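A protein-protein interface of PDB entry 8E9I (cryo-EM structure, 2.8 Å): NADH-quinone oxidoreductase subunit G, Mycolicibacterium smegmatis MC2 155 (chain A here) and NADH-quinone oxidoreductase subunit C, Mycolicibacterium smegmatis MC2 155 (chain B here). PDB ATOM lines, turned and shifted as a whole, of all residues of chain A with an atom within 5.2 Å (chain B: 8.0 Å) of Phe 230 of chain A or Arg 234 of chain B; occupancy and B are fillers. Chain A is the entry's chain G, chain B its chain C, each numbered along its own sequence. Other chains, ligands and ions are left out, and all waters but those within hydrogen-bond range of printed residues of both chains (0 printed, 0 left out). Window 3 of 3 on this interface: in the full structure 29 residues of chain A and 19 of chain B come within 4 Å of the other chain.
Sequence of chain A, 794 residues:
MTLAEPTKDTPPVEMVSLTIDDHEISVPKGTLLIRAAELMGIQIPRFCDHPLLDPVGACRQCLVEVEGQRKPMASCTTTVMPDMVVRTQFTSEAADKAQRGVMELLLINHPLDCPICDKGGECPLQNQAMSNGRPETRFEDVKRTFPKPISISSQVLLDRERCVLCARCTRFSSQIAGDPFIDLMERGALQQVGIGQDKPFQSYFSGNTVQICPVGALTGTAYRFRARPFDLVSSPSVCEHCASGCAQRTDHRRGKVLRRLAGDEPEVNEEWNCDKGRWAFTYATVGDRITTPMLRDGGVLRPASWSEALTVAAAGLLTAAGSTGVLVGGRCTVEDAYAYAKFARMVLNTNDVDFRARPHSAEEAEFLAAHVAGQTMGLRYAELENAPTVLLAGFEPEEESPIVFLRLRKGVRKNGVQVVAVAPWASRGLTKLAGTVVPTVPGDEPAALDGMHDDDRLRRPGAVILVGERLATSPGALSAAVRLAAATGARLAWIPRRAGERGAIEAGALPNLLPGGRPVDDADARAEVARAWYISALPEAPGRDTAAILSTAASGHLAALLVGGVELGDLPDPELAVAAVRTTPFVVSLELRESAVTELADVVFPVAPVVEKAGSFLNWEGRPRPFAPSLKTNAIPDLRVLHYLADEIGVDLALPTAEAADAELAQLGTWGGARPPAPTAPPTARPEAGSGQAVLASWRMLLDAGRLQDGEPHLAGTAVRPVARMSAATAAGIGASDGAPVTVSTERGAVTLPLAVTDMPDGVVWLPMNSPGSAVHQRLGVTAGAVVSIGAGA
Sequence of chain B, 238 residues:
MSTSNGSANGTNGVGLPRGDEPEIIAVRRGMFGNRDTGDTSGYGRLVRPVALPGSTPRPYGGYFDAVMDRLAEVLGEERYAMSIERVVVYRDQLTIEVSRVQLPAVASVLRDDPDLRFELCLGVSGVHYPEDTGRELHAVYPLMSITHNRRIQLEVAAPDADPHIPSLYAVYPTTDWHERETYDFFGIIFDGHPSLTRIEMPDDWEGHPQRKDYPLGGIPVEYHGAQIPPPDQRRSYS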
ATOM      1  N   ARG A 228      13.237   0.624  11.563  1.00  0.00           N
ATOM      2  CA  ARG A 228      13.009   1.952  12.100  1.00  0.00           C
ATOM      3  C   ARG A 228      11.530   2.281  12.048  1.00  0.00           C
ATOM      4  O   ARG A 228      10.777   1.698  11.262  1.00  0.00           O
ATOM      5  CB  ARG A 228      13.796   3.004  11.314  1.00  0.00           C
ATOM      6  CG  ARG A 228      15.219   2.618  10.960  1.00  0.00           C
ATOM      7  CD  ARG A 228      16.011   2.123  12.153  1.00  0.00           C
ATOM      8  NE  ARG A 228      16.267   3.161  13.139  1.00  0.00           N
ATOM      9  CZ  ARG A 228      17.390   3.859  13.224  1.00  0.00           C
ATOM     10  NH1 ARG A 228      18.359   3.725  12.336  1.00  0.00           N
ATOM     11  NH2 ARG A 228      17.548   4.712  14.227  1.00  0.00           N
ATOM     12  N   PRO A 229      11.075   3.238  12.856  1.00  0.00           N
ATOM     13  CA  PRO A 229       9.627   3.462  12.970  1.00  0.00           C
ATOM     14  C   PRO A 229       8.940   3.653  11.635  1.00  0.00           C
ATOM     15  O   PRO A 229       7.838   3.136  11.428  1.00  0.00           O
ATOM     16  CB  PRO A 229       9.547   4.729  13.827  1.00  0.00           C
ATOM     17  CG  PRO A 229      10.787   4.723  14.613  1.00  0.00           C
ATOM     18  CD  PRO A 229      11.839   4.123  13.747  1.00  0.00           C
ATOM     19  N   PHE A 230       9.568   4.369  10.711  1.00  0.00           N
ATOM     20  CA  PHE A 230       8.950   4.603   9.418  1.00  0.00           C
ATOM     21  C   PHE A 230       8.781   3.331   8.603  1.00  0.00           C
ATOM     22  O   PHE A 230       7.964   3.317   7.679  1.00  0.00           O
ATOM     23  CB  PHE A 230       9.784   5.609   8.637  1.00  0.00           C
ATOM     24  CG  PHE A 230      10.839   4.984   7.791  1.00  0.00           C
ATOM     25  CD1 PHE A 230      12.063   4.656   8.328  1.00  0.00           C
ATOM     26  CD2 PHE A 230      10.608   4.722   6.462  1.00  0.00           C
ATOM     27  CE1 PHE A 230      13.033   4.080   7.553  1.00  0.00           C
ATOM     28  CE2 PHE A 230      11.572   4.148   5.689  1.00  0.00           C
ATOM     29  CZ  PHE A 230      12.789   3.826   6.236  1.00  0.00           C
ATOM     30  N   ASP A 231       9.520   2.267   8.911  1.00  0.00           N
ATOM     31  CA  ASP A 231       9.453   1.037   8.132  1.00  0.00           C
ATOM     32  C   ASP A 231       8.415   0.071   8.687  1.00  0.00           C
ATOM     33  O   ASP A 231       8.285  -1.040   8.175  1.00  0.00           O
ATOM     34  CB  ASP A 231      10.822   0.358   8.081  1.00  0.00           C
ATOM     35  N   LEU A 232       7.669   0.473   9.710  1.00  0.00           N
ATOM     36  CA  LEU A 232       6.745  -0.432  10.380  1.00  0.00           C
ATOM     37  C   LEU A 232       5.312  -0.153   9.956  1.00  0.00           C
ATOM     38  O   LEU A 232       4.849   0.988  10.029  1.00  0.00           O
ATOM     39  CB  LEU A 232       6.859  -0.277  11.892  1.00  0.00           C
ATOM     40  CG  LEU A 232       7.940  -1.030  12.651  1.00  0.00           C
ATOM     41  CD1 LEU A 232       9.297  -0.621  12.187  1.00  0.00           C
ATOM     42  CD2 LEU A 232       7.801  -0.714  14.119  1.00  0.00           C
ATOM     43  N   VAL A 233       4.602  -1.193   9.529  1.00  0.00           N
ATOM     44  CA  VAL A 233       3.150  -1.129   9.527  1.00  0.00           C
ATOM     45  C   VAL A 233       2.659  -1.474  10.922  1.00  0.00           C
ATOM     46  O   VAL A 233       2.942  -2.560  11.448  1.00  0.00           O
ATOM     47  CB  VAL A 233       2.551  -2.081   8.479  1.00  0.00           C
ATOM     48  CG1 VAL A 233       1.040  -1.969   8.465  1.00  0.00           C
ATOM     49  CG2 VAL A 233       3.100  -1.780   7.115  1.00  0.00           C
ATOM     50  N   VAL B 221       5.950  -1.138  -2.951  1.00  0.00           N
ATOM     51  CA  VAL B 221       7.122  -1.034  -3.807  1.00  0.00           C
ATOM     52  C   VAL B 221       7.916  -2.324  -3.684  1.00  0.00           C
ATOM     53  O   VAL B 221       8.208  -2.778  -2.574  1.00  0.00           O
ATOM     54  CB  VAL B 221       7.973   0.175  -3.414  1.00  0.00           C
ATOM     55  CG1 VAL B 221       9.177   0.288  -4.324  1.00  0.00           C
ATOM     56  CG2 VAL B 221       7.140   1.436  -3.447  1.00  0.00           C
ATOM     57  N   GLN B 227       9.037  -5.978   0.165  1.00  0.00           N
ATOM     58  CA  GLN B 227       8.254  -4.897  -0.402  1.00  0.00           C
ATOM     59  C   GLN B 227       7.935  -3.891   0.691  1.00  0.00           C
ATOM     60  O   GLN B 227       7.784  -4.246   1.861  1.00  0.00           O
ATOM     61  CB  GLN B 227       6.969  -5.409  -1.045  1.00  0.00           C
ATOM     62  CG  GLN B 227       6.021  -6.059  -0.073  1.00  0.00           C
ATOM     63  CD  GLN B 227       4.767  -6.549  -0.746  1.00  0.00           C
ATOM     64  OE1 GLN B 227       4.690  -6.609  -1.971  1.00  0.00           O
ATOM     65  NE2 GLN B 227       3.769  -6.900   0.051  1.00  0.00           N
ATOM     66  N   ILE B 228       7.836  -2.632   0.294  1.00  0.00           N
ATOM     67  CA  ILE B 228       7.541  -1.525   1.198  1.00  0.00           C
ATOM     68  C   ILE B 228       6.091  -1.111   0.971  1.00  0.00           C
ATOM     69  O   ILE B 228       5.748  -0.679  -0.134  1.00  0.00           O
ATOM     70  CB  ILE B 228       8.490  -0.339   0.973  1.00  0.00           C
ATOM     71  CG1 ILE B 228       9.938  -0.781   1.163  1.00  0.00           C
ATOM     72  CG2 ILE B 228       8.172   0.785   1.934  1.00  0.00           C
ATOM     73  CD1 ILE B 228      10.946   0.310   0.915  1.00  0.00           C
ATOM     74  N   PRO B 229       5.218  -1.213   1.964  1.00  0.00           N
ATOM     75  CA  PRO B 229       3.844  -0.754   1.786  1.00  0.00           C
ATOM     76  C   PRO B 229       3.798   0.745   1.558  1.00  0.00           C
ATOM     77  O   PRO B 229       4.739   1.466   1.920  1.00  0.00           O
ATOM     78  CB  PRO B 229       3.174  -1.135   3.111  1.00  0.00           C
ATOM     79  CG  PRO B 229       4.011  -2.228   3.645  1.00  0.00           C
ATOM     80  CD  PRO B 229       5.398  -1.873   3.264  1.00  0.00           C
ATOM     81  N   PRO B 230       2.723   1.255   0.966  1.00  0.00           N
ATOM     82  CA  PRO B 230       2.636   2.690   0.688  1.00  0.00           C
ATOM     83  C   PRO B 230       2.816   3.501   1.957  1.00  0.00           C
ATOM     84  O   PRO B 230       2.749   2.957   3.068  1.00  0.00           O
ATOM     85  CB  PRO B 230       1.222   2.860   0.119  1.00  0.00           C
ATOM     86  CG  PRO B 230       0.831   1.513  -0.346  1.00  0.00           C
ATOM     87  CD  PRO B 230       1.500   0.544   0.564  1.00  0.00           C
ATOM     88  N   PRO B 231       3.059   4.807   1.834  1.00  0.00           N
ATOM     89  CA  PRO B 231       3.261   5.636   3.030  1.00  0.00           C
ATOM     90  C   PRO B 231       2.051   5.719   3.944  1.00  0.00           C
ATOM     91  O   PRO B 231       2.230   5.971   5.141  1.00  0.00           O
ATOM     92  CB  PRO B 231       3.604   7.007   2.444  1.00  0.00           C
ATOM     93  CG  PRO B 231       2.961   7.007   1.118  1.00  0.00           C
ATOM     94  CD  PRO B 231       3.121   5.609   0.605  1.00  0.00           C
ATOM     95  N   ASP B 232       0.836   5.536   3.436  1.00  0.00           N
ATOM     96  CA  ASP B 232      -0.339   5.672   4.284  1.00  0.00           C
ATOM     97  C   ASP B 232      -0.524   4.494   5.224  1.00  0.00           C
ATOM     98  O   ASP B 232      -1.281   4.606   6.191  1.00  0.00           O
ATOM     99  CB  ASP B 232      -1.597   5.832   3.436  1.00  0.00           C
ATOM    100  CG  ASP B 232      -2.016   4.541   2.774  1.00  0.00           C
ATOM    101  OD1 ASP B 232      -1.126   3.762   2.389  1.00  0.00           O
ATOM    102  OD2 ASP B 232      -3.235   4.300   2.649  1.00  0.00           O
ATOM    103  N   GLN B 233       0.135   3.370   4.958  1.00  0.00           N
ATOM    104  CA  GLN B 233       0.013   2.213   5.833  1.00  0.00           C
ATOM    105  C   GLN B 233       1.066   2.228   6.930  1.00  0.00           C
ATOM    106  O   GLN B 233       0.791   1.826   8.063  1.00  0.00           O
ATOM    107  CB  GLN B 233       0.130   0.932   5.016  1.00  0.00           C
ATOM    108  CG  GLN B 233      -0.887   0.823   3.911  1.00  0.00           C
ATOM    109  CD  GLN B 233      -0.820  -0.504   3.203  1.00  0.00           C
ATOM    110  OE1 GLN B 233      -0.154  -1.428   3.656  1.00  0.00           O
ATOM    111  NE2 GLN B 233      -1.515  -0.609   2.080  1.00  0.00           N
ATOM    112  N   ARG B 234       2.269   2.684   6.613  1.00  0.00           N
ATOM    113  CA  ARG B 234       3.357   2.637   7.567  1.00  0.00           C
ATOM    114  C   ARG B 234       3.206   3.735   8.608  1.00  0.00           C
ATOM    115  O   ARG B 234       2.408   4.663   8.467  1.00  0.00           O
ATOM    116  CB  ARG B 234       4.693   2.757   6.848  1.00  0.00           C
ATOM    117  CG  ARG B 234       4.846   1.758   5.714  1.00  0.00           C
ATOM    118  CD  ARG B 234       6.268   1.678   5.239  1.00  0.00           C
ATOM    119  NE  ARG B 234       6.904   2.986   5.307  1.00  0.00           N
ATOM    120  CZ  ARG B 234       6.934   3.862   4.315  1.00  0.00           C
ATOM    121  NH1 ARG B 234       6.371   3.606   3.147  1.00  0.00           N
ATOM    122  NH2 ARG B 234       7.535   5.031   4.504  1.00  0.00           N
ATOM    123  N   ARG B 235       4.000   3.613   9.668  1.00  0.00           N
ATOM    124  CA  ARG B 235       3.852   4.469  10.833  1.00  0.00           C
ATOM    125  C   ARG B 235       4.179   5.920  10.502  1.00  0.00           C
ATOM    126  O   ARG B 235       4.920   6.219   9.563  1.00  0.00           O
ATOM    127  CB  ARG B 235       4.757   3.973  11.956  1.00  0.00           C
ATOM    128  CG  ARG B 235       4.484   4.632  13.279  1.00  0.00           C
ATOM    129  CD  ARG B 235       5.019   3.818  14.435  1.00  0.00           C
ATOM    130  NE  ARG B 235       4.601   4.398  15.700  1.00  0.00           N
ATOM    131  CZ  ARG B 235       3.350   4.406  16.137  1.00  0.00           C
ATOM    132  NH1 ARG B 235       2.376   3.835  15.452  1.00  0.00           N
ATOM    133  NH2 ARG B 235       3.070   5.005  17.290  1.00  0.00           N
ATOM    134  N   SER B 236       3.607   6.826  11.292  1.00  0.00           N
ATOM    135  CA  SER B 236       3.795   8.253  11.089  1.00  0.00           C
ATOM    136  C   SER B 236       3.653   8.964  12.423  1.00  0.00           C
ATOM    137  O   SER B 236       3.086   8.429  13.377  1.00  0.00           O
ATOM    138  CB  SER B 236       2.781   8.819  10.097  1.00  0.00           C
ATOM    139  OG  SER B 236       1.468   8.677  10.599  1.00  0.00           O
ATOM    140  N   TYR B 237       4.170  10.186  12.475  1.00  0.00           N
ATOM    141  CA  TYR B 237       4.040  11.015  13.662  1.00  0.00           C
ATOM    142  C   TYR B 237       3.697  12.445  13.271  1.00  0.00           C
ATOM    143  O   TYR B 237       4.109  13.395  13.931  1.00  0.00           O
ATOM    144  CB  TYR B 237       5.326  10.977  14.479  1.00  0.00           C
ATOM    145  CG  TYR B 237       5.722   9.582  14.898  1.00  0.00           C
ATOM    146  CD1 TYR B 237       6.485   8.779  14.066  1.00  0.00           C
ATOM    147  CD2 TYR B 237       5.330   9.066  16.121  1.00  0.00           C
ATOM    148  CE1 TYR B 237       6.844   7.506  14.437  1.00  0.00           C
ATOM    149  CE2 TYR B 237       5.687   7.793  16.502  1.00  0.00           C
ATOM    150  CZ  TYR B 237       6.445   7.019  15.656  1.00  0.00           C
ATOM    151  OH  TYR B 237       6.800   5.748  16.034  1.00  0.00           O
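NE of Arg 234 of chain B lies within hydrogen-bond range of O of Phe 230 of chain A, 2.6 Å away. The backbone carbonyl oxygen (O) of Leu 232 of chain A sits at hydrogen-bond distance from the backbone NH (N) of Arg 235 of chain B (2.8 Å).
The backbone carbonyl oxygen (O) of Pro 229 of chain B sits at hydrogen-bond distance from the guanidinium group (NH1) of Arg 234 of chain B (3.0 Å). OH of Tyr 237 of chain B is in hydrogen-bond range of NE of Arg 235 of chain B, at 2.6 Å.
Among the printed residues, pairs that only touch across the chains: Pro 229 of chain A with Arg 235 of chain B (3.2 Å), Pro 229 of chain A with Tyr 237 of chain B (3.7 Å), Leu 232 of chain A with Arg 234 of chain B (3.3 Å), Val 233 of chain A with Pro 229 of chain B (3.6 Å) and Val 233 of chain A with Gln 233 of chain B (3.8 Å).
Of the printed residues of chain B, Pro 229 of chain A touches Arg 235 (3.2 Å) and Tyr 237 (3.7 Å). Of the printed residues of chain B, Phe 230 of chain A touches Arg 234. Of chain A, only Phe 230 (2.6 Å) and Leu 232 (3.3 Å) come within 4 Å of Arg 234 of chain B. Of the printed residues of chain A, Tyr 237 of chain B touches Pro 229 (3.7 Å). The nearest printed residue of chain B that does not touch Leu 232 of chain A is Gln 233 of chain B (4.6 Å).
Of the 6 printed residues of chain A, 4 touch a printed residue of chain B. Hydrophobic or aromatic side chains of chain A that line the printed part of chain B: Pro 229, Phe 230 and Val 233. Among the printed residues, no Asp or Glu carboxylate lies within 4 Å of a Lys or Arg side-chain nitrogen of the other chain.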
